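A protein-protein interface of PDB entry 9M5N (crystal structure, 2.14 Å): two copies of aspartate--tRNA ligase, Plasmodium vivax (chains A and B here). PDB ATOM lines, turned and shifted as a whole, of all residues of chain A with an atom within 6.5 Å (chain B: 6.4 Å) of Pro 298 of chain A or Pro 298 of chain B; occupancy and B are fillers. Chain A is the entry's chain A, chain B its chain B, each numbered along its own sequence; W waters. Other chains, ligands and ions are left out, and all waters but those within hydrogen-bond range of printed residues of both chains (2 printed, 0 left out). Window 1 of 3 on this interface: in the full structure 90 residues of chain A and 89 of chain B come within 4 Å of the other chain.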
ATOM      1  N   HIS A 247      23.872 -26.572   3.188  1.00  0.00           N
ATOM      2  CA  HIS A 247      24.104 -25.535   2.190  1.00  0.00           C
ATOM      3  C   HIS A 247      24.491 -26.213   0.891  1.00  0.00           C
ATOM      4  O   HIS A 247      25.496 -26.939   0.843  1.00  0.00           O
ATOM      5  CB  HIS A 247      25.190 -24.554   2.648  1.00  0.00           C
ATOM      6  CG  HIS A 247      24.813 -23.794   3.886  1.00  0.00           C
ATOM      7  ND1 HIS A 247      23.996 -22.684   3.855  1.00  0.00           N
ATOM      8  CD2 HIS A 247      25.087 -24.024   5.194  1.00  0.00           C
ATOM      9  CE1 HIS A 247      23.803 -22.245   5.089  1.00  0.00           C
ATOM     10  NE2 HIS A 247      24.460 -23.036   5.918  1.00  0.00           N
ATOM     11  N   THR A 248      23.674 -26.013  -0.141  1.00  0.00           N
ATOM     12  CA  THR A 248      23.804 -26.716  -1.404  1.00  0.00           C
ATOM     13  C   THR A 248      24.032 -25.710  -2.526  1.00  0.00           C
ATOM     14  O   THR A 248      23.662 -24.538  -2.387  1.00  0.00           O
ATOM     15  CB  THR A 248      22.554 -27.572  -1.683  1.00  0.00           C
ATOM     16  OG1 THR A 248      21.394 -26.737  -1.794  1.00  0.00           O
ATOM     17  CG2 THR A 248      22.345 -28.578  -0.533  1.00  0.00           C
ATOM     18  N   LYS A 250      24.275 -23.183  -5.742  1.00  0.00           N
ATOM     19  CA  LYS A 250      23.387 -22.473  -6.655  1.00  0.00           C
ATOM     20  C   LYS A 250      23.910 -22.436  -8.081  1.00  0.00           C
ATOM     21  O   LYS A 250      23.137 -22.140  -8.995  1.00  0.00           O
ATOM     22  CB  LYS A 250      23.145 -21.034  -6.181  1.00  0.00           C
ATOM     23  CG  LYS A 250      22.859 -20.910  -4.690  1.00  0.00           C
ATOM     24  CD  LYS A 250      21.697 -21.808  -4.270  1.00  0.00           C
ATOM     25  CE  LYS A 250      21.680 -22.004  -2.746  1.00  0.00           C
ATOM     26  NZ  LYS A 250      20.917 -23.221  -2.342  1.00  0.00           N
ATOM     27  N   ALA A 275      20.451 -22.008  -9.662  1.00  0.00           N
ATOM     28  CA  ALA A 275      19.427 -22.853  -9.059  1.00  0.00           C
ATOM     29  C   ALA A 275      18.133 -22.067  -8.865  1.00  0.00           C
ATOM     30  O   ALA A 275      18.139 -20.946  -8.348  1.00  0.00           O
ATOM     31  CB  ALA A 275      19.914 -23.413  -7.720  1.00  0.00           C
ATOM     32  N   SER A 277      15.888 -23.687  -7.126  1.00  0.00           N
ATOM     33  CA  SER A 277      15.464 -24.476  -5.990  1.00  0.00           C
ATOM     34  C   SER A 277      16.591 -25.420  -5.601  1.00  0.00           C
ATOM     35  O   SER A 277      17.332 -25.894  -6.476  1.00  0.00           O
ATOM     36  CB  SER A 277      14.210 -25.277  -6.335  1.00  0.00           C
ATOM     37  OG  SER A 277      13.948 -26.193  -5.299  1.00  0.00           O
ATOM     38  N   PRO A 278      16.755 -25.715  -4.312  1.00  0.00           N
ATOM     39  CA  PRO A 278      17.736 -26.721  -3.897  1.00  0.00           C
ATOM     40  C   PRO A 278      17.157 -28.135  -3.912  1.00  0.00           C
ATOM     41  O   PRO A 278      17.753 -29.053  -3.341  1.00  0.00           O
ATOM     42  CB  PRO A 278      18.077 -26.276  -2.473  1.00  0.00           C
ATOM     43  CG  PRO A 278      16.729 -25.804  -1.963  1.00  0.00           C
ATOM     44  CD  PRO A 278      16.103 -25.081  -3.150  1.00  0.00           C
ATOM     45  N   GLU A 295      17.322 -25.838   4.638  1.00  0.00           N
ATOM     46  CA  GLU A 295      18.225 -24.847   4.071  1.00  0.00           C
ATOM     47  C   GLU A 295      17.492 -23.516   3.988  1.00  0.00           C
ATOM     48  O   GLU A 295      16.294 -23.481   3.711  1.00  0.00           O
ATOM     49  CB  GLU A 295      18.742 -25.263   2.675  1.00  0.00           C
ATOM     50  CG  GLU A 295      19.671 -24.228   2.011  1.00  0.00           C
ATOM     51  CD  GLU A 295      20.490 -24.813   0.861  1.00  0.00           C
ATOM     52  OE1 GLU A 295      21.439 -24.132   0.387  1.00  0.00           O
ATOM     53  OE2 GLU A 295      20.191 -25.956   0.434  1.00  0.00           O
ATOM     54  N   VAL A 296      18.208 -22.431   4.264  1.00  0.00           N
ATOM     55  CA  VAL A 296      17.707 -21.064   4.155  1.00  0.00           C
ATOM     56  C   VAL A 296      18.657 -20.384   3.199  1.00  0.00           C
ATOM     57  O   VAL A 296      19.818 -20.157   3.551  1.00  0.00           O
ATOM     58  CB  VAL A 296      17.684 -20.344   5.509  1.00  0.00           C
ATOM     59  CG1 VAL A 296      17.200 -18.892   5.346  1.00  0.00           C
ATOM     60  CG2 VAL A 296      16.813 -21.107   6.494  1.00  0.00           C
ATOM     61  N   ALA A 297      18.208 -20.095   1.983  1.00  0.00           N
ATOM     62  CA  ALA A 297      19.178 -19.697   0.966  1.00  0.00           C
ATOM     63  C   ALA A 297      18.448 -19.053  -0.208  1.00  0.00           C
ATOM     64  O   ALA A 297      17.263 -19.312  -0.425  1.00  0.00           O
ATOM     65  CB  ALA A 297      20.016 -20.899   0.491  1.00  0.00           C
ATOM     66  N   PRO A 298      19.140 -18.219  -0.973  1.00  0.00           N
ATOM     67  CA  PRO A 298      18.503 -17.616  -2.144  1.00  0.00           C
ATOM     68  C   PRO A 298      18.276 -18.639  -3.242  1.00  0.00           C
ATOM     69  O   PRO A 298      19.017 -19.613  -3.383  1.00  0.00           O
ATOM     70  CB  PRO A 298      19.513 -16.549  -2.594  1.00  0.00           C
ATOM     71  CG  PRO A 298      20.812 -16.971  -1.997  1.00  0.00           C
ATOM     72  CD  PRO A 298      20.466 -17.633  -0.699  1.00  0.00           C
ATOM     73  N   VAL A 299      17.226 -18.396  -4.020  1.00  0.00           N
ATOM     74  CA  VAL A 299      16.992 -19.055  -5.298  1.00  0.00           C
ATOM     75  C   VAL A 299      16.686 -17.974  -6.328  1.00  0.00           C
ATOM     76  O   VAL A 299      16.355 -16.829  -5.991  1.00  0.00           O
ATOM     77  CB  VAL A 299      15.852 -20.086  -5.230  1.00  0.00           C
ATOM     78  CG1 VAL A 299      16.102 -21.082  -4.100  1.00  0.00           C
ATOM     79  CG2 VAL A 299      14.524 -19.364  -5.005  1.00  0.00           C
ATOM     80  N   PHE A 300      16.811 -18.356  -7.598  1.00  0.00           N
ATOM     81  CA  PHE A 300      16.817 -17.419  -8.712  1.00  0.00           C
ATOM     82  C   PHE A 300      15.852 -17.908  -9.783  1.00  0.00           C
ATOM     83  O   PHE A 300      15.959 -19.053 -10.243  1.00  0.00           O
ATOM     84  CB  PHE A 300      18.231 -17.271  -9.273  1.00  0.00           C
ATOM     85  CG  PHE A 300      19.270 -17.030  -8.213  1.00  0.00           C
ATOM     86  CD1 PHE A 300      19.611 -15.734  -7.835  1.00  0.00           C
ATOM     87  CD2 PHE A 300      19.901 -18.103  -7.584  1.00  0.00           C
ATOM     88  CE1 PHE A 300      20.577 -15.511  -6.860  1.00  0.00           C
ATOM     89  CE2 PHE A 300      20.866 -17.897  -6.601  1.00  0.00           C
ATOM     90  CZ  PHE A 300      21.210 -16.594  -6.238  1.00  0.00           C
ATOM     91  N   GLU A 313      14.619 -13.007  -7.554  1.00  0.00           N
ATOM     92  CA  GLU A 313      15.491 -13.597  -6.554  1.00  0.00           C
ATOM     93  C   GLU A 313      14.734 -13.583  -5.235  1.00  0.00           C
ATOM     94  O   GLU A 313      14.138 -12.559  -4.887  1.00  0.00           O
ATOM     95  CB  GLU A 313      16.807 -12.807  -6.429  1.00  0.00           C
ATOM     96  CG  GLU A 313      17.736 -13.298  -5.307  1.00  0.00           C
ATOM     97  CD  GLU A 313      19.131 -12.656  -5.333  1.00  0.00           C
ATOM     98  OE1 GLU A 313      19.456 -11.871  -6.261  1.00  0.00           O
ATOM     99  OE2 GLU A 313      19.908 -12.943  -4.411  1.00  0.00           O
ATOM    100  N   TYR A 314      14.728 -14.695  -4.506  1.00  0.00           N
ATOM    101  CA  TYR A 314      14.114 -14.622  -3.179  1.00  0.00           C
ATOM    102  C   TYR A 314      14.788 -15.620  -2.255  1.00  0.00           C
ATOM    103  O   TYR A 314      15.634 -16.405  -2.680  1.00  0.00           O
ATOM    104  CB  TYR A 314      12.584 -14.830  -3.232  1.00  0.00           C
ATOM    105  CG  TYR A 314      12.101 -16.237  -3.566  1.00  0.00           C
ATOM    106  CD1 TYR A 314      11.718 -17.129  -2.566  1.00  0.00           C
ATOM    107  CD2 TYR A 314      11.991 -16.650  -4.883  1.00  0.00           C
ATOM    108  CE1 TYR A 314      11.251 -18.418  -2.879  1.00  0.00           C
ATOM    109  CE2 TYR A 314      11.525 -17.913  -5.207  1.00  0.00           C
ATOM    110  CZ  TYR A 314      11.159 -18.799  -4.211  1.00  0.00           C
ATOM    111  OH  TYR A 314      10.719 -20.067  -4.550  1.00  0.00           O
ATOM    112  N   VAL A 315      14.443 -15.556  -0.970  1.00  0.00           N
ATOM    113  CA  VAL A 315      14.990 -16.477   0.030  1.00  0.00           C
ATOM    114  C   VAL A 315      14.024 -17.648   0.192  1.00  0.00           C
ATOM    115  O   VAL A 315      12.876 -17.476   0.619  1.00  0.00           O
ATOM    116  CB  VAL A 315      15.228 -15.779   1.375  1.00  0.00           C
ATOM    117  CG1 VAL A 315      15.852 -16.754   2.374  1.00  0.00           C
ATOM    118  CG2 VAL A 315      16.099 -14.533   1.188  1.00  0.00           C
ATOM    119  N   SER A 316      14.483 -18.839  -0.151  1.00  0.00           N
ATOM    120  CA  SER A 316      13.699 -20.054   0.014  1.00  0.00           C
ATOM    121  C   SER A 316      14.060 -20.714   1.341  1.00  0.00           C
ATOM    122  O   SER A 316      15.247 -20.833   1.680  1.00  0.00           O
ATOM    123  CB  SER A 316      13.956 -21.013  -1.145  1.00  0.00           C
ATOM    124  OG  SER A 316      13.017 -22.082  -1.133  1.00  0.00           O
ATOM    125  N   HIS B 247      19.084 -10.629   4.457  1.00  0.00           N
ATOM    126  CA  HIS B 247      19.266 -11.362   3.211  1.00  0.00           C
ATOM    127  C   HIS B 247      19.329 -10.343   2.092  1.00  0.00           C
ATOM    128  O   HIS B 247      18.347  -9.630   1.840  1.00  0.00           O
ATOM    129  CB  HIS B 247      18.125 -12.357   2.980  1.00  0.00           C
ATOM    130  CG  HIS B 247      18.021 -13.412   4.039  1.00  0.00           C
ATOM    131  ND1 HIS B 247      18.812 -14.544   4.041  1.00  0.00           N
ATOM    132  CD2 HIS B 247      17.224 -13.504   5.134  1.00  0.00           C
ATOM    133  CE1 HIS B 247      18.499 -15.292   5.086  1.00  0.00           C
ATOM    134  NE2 HIS B 247      17.539 -14.683   5.764  1.00  0.00           N
ATOM    135  N   THR B 248      20.472 -10.274   1.423  1.00  0.00           N
ATOM    136  CA  THR B 248      20.741  -9.266   0.410  1.00  0.00           C
ATOM    137  C   THR B 248      21.007  -9.959  -0.923  1.00  0.00           C
ATOM    138  O   THR B 248      21.379 -11.143  -0.947  1.00  0.00           O
ATOM    139  CB  THR B 248      21.945  -8.405   0.826  1.00  0.00           C
ATOM    140  OG1 THR B 248      23.124  -9.217   0.849  1.00  0.00           O
ATOM    141  CG2 THR B 248      21.735  -7.826   2.239  1.00  0.00           C
ATOM    142  N   LYS B 250      22.130 -11.545  -4.543  1.00  0.00           N
ATOM    143  CA  LYS B 250      23.329 -12.038  -5.202  1.00  0.00           C
ATOM    144  C   LYS B 250      23.356 -11.707  -6.693  1.00  0.00           C
ATOM    145  O   LYS B 250      24.410 -11.861  -7.328  1.00  0.00           O
ATOM    146  CB  LYS B 250      23.469 -13.555  -4.996  1.00  0.00           C
ATOM    147  CG  LYS B 250      23.184 -14.033  -3.560  1.00  0.00           C
ATOM    148  CD  LYS B 250      23.933 -13.234  -2.487  1.00  0.00           C
ATOM    149  CE  LYS B 250      23.326 -13.529  -1.096  1.00  0.00           C
ATOM    150  NZ  LYS B 250      23.796 -12.561  -0.042  1.00  0.00           N
ATOM    151  N   ALA B 275      27.183 -11.855  -6.941  1.00  0.00           N
ATOM    152  CA  ALA B 275      27.861 -11.257  -5.803  1.00  0.00           C
ATOM    153  C   ALA B 275      29.043 -12.120  -5.375  1.00  0.00           C
ATOM    154  O   ALA B 275      28.903 -13.330  -5.192  1.00  0.00           O
ATOM    155  CB  ALA B 275      26.887 -11.090  -4.636  1.00  0.00           C
ATOM    156  N   SER B 277      30.352 -11.068  -2.569  1.00  0.00           N
ATOM    157  CA  SER B 277      30.282 -10.708  -1.167  1.00  0.00           C
ATOM    158  C   SER B 277      29.043  -9.844  -0.995  1.00  0.00           C
ATOM    159  O   SER B 277      28.642  -9.170  -1.948  1.00  0.00           O
ATOM    160  CB  SER B 277      31.551  -9.960  -0.753  1.00  0.00           C
ATOM    161  OG  SER B 277      31.329  -9.142   0.370  1.00  0.00           O
ATOM    162  N   PRO B 278      28.400  -9.846   0.175  1.00  0.00           N
ATOM    163  CA  PRO B 278      27.295  -8.911   0.405  1.00  0.00           C
ATOM    164  C   PRO B 278      27.783  -7.574   0.955  1.00  0.00           C
ATOM    165  O   PRO B 278      26.988  -6.820   1.519  1.00  0.00           O
ATOM    166  CB  PRO B 278      26.439  -9.653   1.435  1.00  0.00           C
ATOM    167  CG  PRO B 278      27.490 -10.333   2.293  1.00  0.00           C
ATOM    168  CD  PRO B 278      28.588 -10.756   1.323  1.00  0.00           C
ATOM    169  N   GLU B 295      24.647 -11.996   7.844  1.00  0.00           N
ATOM    170  CA  GLU B 295      24.096 -12.794   6.760  1.00  0.00           C
ATOM    171  C   GLU B 295      24.850 -14.124   6.680  1.00  0.00           C
ATOM    172  O   GLU B 295      26.061 -14.176   6.899  1.00  0.00           O
ATOM    173  CB  GLU B 295      24.166 -12.036   5.415  1.00  0.00           C
ATOM    174  CG  GLU B 295      23.454 -12.750   4.263  1.00  0.00           C
ATOM    175  CD  GLU B 295      23.128 -11.841   3.089  1.00  0.00           C
ATOM    176  OE1 GLU B 295      23.510 -10.648   3.105  1.00  0.00           O
ATOM    177  OE2 GLU B 295      22.482 -12.322   2.137  1.00  0.00           O
ATOM    178  N   VAL B 296      24.119 -15.203   6.405  1.00  0.00           N
ATOM    179  CA  VAL B 296      24.681 -16.531   6.141  1.00  0.00           C
ATOM    180  C   VAL B 296      24.199 -16.907   4.751  1.00  0.00           C
ATOM    181  O   VAL B 296      23.015 -17.204   4.573  1.00  0.00           O
ATOM    182  CB  VAL B 296      24.238 -17.556   7.201  1.00  0.00           C
ATOM    183  CG1 VAL B 296      24.820 -18.942   6.942  1.00  0.00           C
ATOM    184  CG2 VAL B 296      24.627 -17.081   8.614  1.00  0.00           C
ATOM    185  N   ALA B 297      25.072 -16.838   3.744  1.00  0.00           N
ATOM    186  CA  ALA B 297      24.537 -16.988   2.398  1.00  0.00           C
ATOM    187  C   ALA B 297      25.665 -17.337   1.438  1.00  0.00           C
ATOM    188  O   ALA B 297      26.839 -17.086   1.735  1.00  0.00           O
ATOM    189  CB  ALA B 297      23.807 -15.702   1.934  1.00  0.00           C
ATOM    190  N   PRO B 298      25.336 -17.885   0.264  1.00  0.00           N
ATOM    191  CA  PRO B 298      26.367 -18.150  -0.750  1.00  0.00           C
ATOM    192  C   PRO B 298      27.001 -16.876  -1.283  1.00  0.00           C
ATOM    193  O   PRO B 298      26.364 -15.824  -1.365  1.00  0.00           O
ATOM    194  CB  PRO B 298      25.604 -18.862  -1.872  1.00  0.00           C
ATOM    195  CG  PRO B 298      24.259 -19.174  -1.336  1.00  0.00           C
ATOM    196  CD  PRO B 298      23.988 -18.294  -0.179  1.00  0.00           C
ATOM    197  N   VAL B 299      28.275 -16.997  -1.668  1.00  0.00           N
ATOM    198  CA  VAL B 299      28.941 -16.051  -2.553  1.00  0.00           C
ATOM    199  C   VAL B 299      29.598 -16.844  -3.675  1.00  0.00           C
ATOM    200  O   VAL B 299      29.790 -18.068  -3.585  1.00  0.00           O
ATOM    201  CB  VAL B 299      29.991 -15.187  -1.830  1.00  0.00           C
ATOM    202  CG1 VAL B 299      29.349 -14.376  -0.706  1.00  0.00           C
ATOM    203  CG2 VAL B 299      31.096 -16.080  -1.301  1.00  0.00           C
ATOM    204  N   PHE B 300      29.996 -16.112  -4.715  1.00  0.00           N
ATOM    205  CA  PHE B 300      30.433 -16.700  -5.973  1.00  0.00           C
ATOM    206  C   PHE B 300      31.683 -15.976  -6.449  1.00  0.00           C
ATOM    207  O   PHE B 300      31.678 -14.752  -6.597  1.00  0.00           O
ATOM    208  CB  PHE B 300      29.323 -16.618  -7.021  1.00  0.00           C
ATOM    209  CG  PHE B 300      27.993 -17.040  -6.500  1.00  0.00           C
ATOM    210  CD1 PHE B 300      27.617 -18.377  -6.528  1.00  0.00           C
ATOM    211  CD2 PHE B 300      27.122 -16.105  -5.946  1.00  0.00           C
ATOM    212  CE1 PHE B 300      26.380 -18.791  -6.012  1.00  0.00           C
ATOM    213  CE2 PHE B 300      25.891 -16.506  -5.430  1.00  0.00           C
ATOM    214  CZ  PHE B 300      25.516 -17.859  -5.468  1.00  0.00           C
ATOM    215  N   GLU B 313      32.290 -21.330  -5.240  1.00  0.00           N
ATOM    216  CA  GLU B 313      31.077 -20.960  -4.538  1.00  0.00           C
ATOM    217  C   GLU B 313      31.237 -21.417  -3.102  1.00  0.00           C
ATOM    218  O   GLU B 313      31.647 -22.555  -2.852  1.00  0.00           O
ATOM    219  CB  GLU B 313      29.837 -21.594  -5.173  1.00  0.00           C
ATOM    220  CG  GLU B 313      28.600 -21.429  -4.312  1.00  0.00           C
ATOM    221  CD  GLU B 313      27.339 -22.025  -4.937  1.00  0.00           C
ATOM    222  OE1 GLU B 313      27.412 -22.594  -6.060  1.00  0.00           O
ATOM    223  OE2 GLU B 313      26.271 -21.921  -4.286  1.00  0.00           O
ATOM    224  N   TYR B 314      30.938 -20.542  -2.154  1.00  0.00           N
ATOM    225  CA  TYR B 314      31.057 -21.002  -0.778  1.00  0.00           C
ATOM    226  C   TYR B 314      30.062 -20.237   0.067  1.00  0.00           C
ATOM    227  O   TYR B 314      29.380 -19.332  -0.417  1.00  0.00           O
ATOM    228  CB  TYR B 314      32.494 -20.870  -0.261  1.00  0.00           C
ATOM    229  CG  TYR B 314      32.967 -19.458  -0.007  1.00  0.00           C
ATOM    230  CD1 TYR B 314      32.798 -18.869   1.250  1.00  0.00           C
ATOM    231  CD2 TYR B 314      33.626 -18.730  -0.997  1.00  0.00           C
ATOM    232  CE1 TYR B 314      33.243 -17.568   1.511  1.00  0.00           C
ATOM    233  CE2 TYR B 314      34.081 -17.418  -0.749  1.00  0.00           C
ATOM    234  CZ  TYR B 314      33.876 -16.848   0.508  1.00  0.00           C
ATOM    235  OH  TYR B 314      34.294 -15.571   0.773  1.00  0.00           O
ATOM    236  N   VAL B 315      29.933 -20.648   1.324  1.00  0.00           N
ATOM    237  CA  VAL B 315      29.001 -20.013   2.245  1.00  0.00           C
ATOM    238  C   VAL B 315      29.763 -18.994   3.070  1.00  0.00           C
ATOM    239  O   VAL B 315      30.673 -19.352   3.826  1.00  0.00           O
ATOM    240  CB  VAL B 315      28.300 -21.036   3.144  1.00  0.00           C
ATOM    241  CG1 VAL B 315      27.337 -20.317   4.059  1.00  0.00           C
ATOM    242  CG2 VAL B 315      27.575 -22.069   2.290  1.00  0.00           C
ATOM    243  N   SER B 316      29.399 -17.726   2.917  1.00  0.00           N
ATOM    244  CA  SER B 316      30.011 -16.639   3.660  1.00  0.00           C
ATOM    245  C   SER B 316      29.155 -16.306   4.874  1.00  0.00           C
ATOM    246  O   SER B 316      27.930 -16.153   4.753  1.00  0.00           O
ATOM    247  CB  SER B 316      30.172 -15.403   2.784  1.00  0.00           C
ATOM    248  OG  SER B 316      30.936 -14.448   3.494  1.00  0.00           O
HETATM  249  O   HOH W   1      20.867 -17.074   2.605  1.00  0.00           O
HETATM  250  O   HOH W   2      22.263 -19.925   2.543  1.00  0.00           O
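The backbone NH of Lys 250 of chain A lies within hydrogen-bond range of the side-chain carboxylate of Glu 313 of chain B.
The backbone NH of Lys 250 of chain B lies within hydrogen-bond range of the side-chain carboxylate of Glu 313 of chain A, 2.6 Å away.
O of Thr 248 of chain A sits at hydrogen-bond distance from NZ of Lys 250 of chain A, 3.0 Å away.
The backbone NH (N) of Ala 275 of chain A lies within hydrogen-bond range of the backbone carbonyl oxygen (O) of Lys 250 of chain A.
The side-chain amino group (NZ) of Lys 250 of chain A is in salt-bridge range of the side-chain carboxylate (OE1) of Glu 295 of chain A (2.9 Å).
The backbone carbonyl oxygen (O) of Lys 250 of chain B sits at hydrogen-bond distance from the backbone NH (N) of Ala 275 of chain B.
OE2 of Glu 295 of chain B lies within salt-bridge range of NZ of Lys 250 of chain B (2.6 Å).
O of Ala 275 of chain B sits at hydrogen-bond distance from N of Phe 300 of chain B (3.0 Å).
Val 296 of chain B touches His 247 of chain A (CG1 to CE1, 3.9 Å).
Val 315 of chain B touches His 247 of chain A.
Lys 250 of chain A touches Phe 300 of chain B.
Val 296 of chain A touches His 247 of chain B (CG1 to CE1, 3.8 Å).
Pro 298 of chain B touches Pro 298 of chain A.
Phe 300 of chain A touches Lys 250 of chain B.
His 247 of chain B touches Val 315 of chain A.
Of the printed residues of chain B, Lys 250 of chain A touches Phe 300 and Glu 313.
Pro 298 of chain A touches just one residue of chain B: Pro 298 (3.6 Å).
Of the printed residues of chain B, Phe 300 of chain A touches Lys 250 (3.96 Å).
Of the printed residues of chain A, His 247 of chain B touches Val 296 and Val 315.
Thr 248 of chain B touches none of the printed residues of chain A.
Of the printed residues of chain A, Lys 250 of chain B touches Phe 300 (3.96 Å) and Glu 313 (2.6 Å).
Pro 298 of chain B touches just one residue of chain A: Pro 298.
The nearest residue of chain A that does not touch Pro 298 of chain B is Lys 250 of chain A (4.03 Å).
Of the 16 printed residues of chain A, 7 touch a printed residue of chain B.
Printed residues of chain A that touch a printed residue of chain B: His 247, Lys 250, Val 296, Pro 298, Phe 300, Glu 313 and Val 315.
Along chain B the printed residues that touch a printed residue of chain A span positions 247 to 315.
Among the printed residues, no Asp or Glu carboxylate lies within 4 Å of a Lys or Arg side-chain nitrogen of the other chain.
His 247 of chain A touches Val 315 of chain B, and with the chains exchanged Val 315 of chain A touches His 247 of chain B.
Lys 250 of chain A touches Phe 300 of chain B, and with the chains exchanged Phe 300 of chain A touches Lys 250 of chain B.
Lys 250 of chain A touches Glu 313 of chain B, and with the chains exchanged Glu 313 of chain A touches Lys 250 of chain B.
Pro 298 of chain B touches its own counterpart, Pro 298 of chain A.
16 positions are printed for both chains.
Water W2 bridges O of Val 296 of chain A and O of Val 296 of chain B.
Water W1 lies within hydrogen-bond range of O of Val 296 of chain B (2.9 Å) and O of Val 296 of chain A (3.4 Å).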
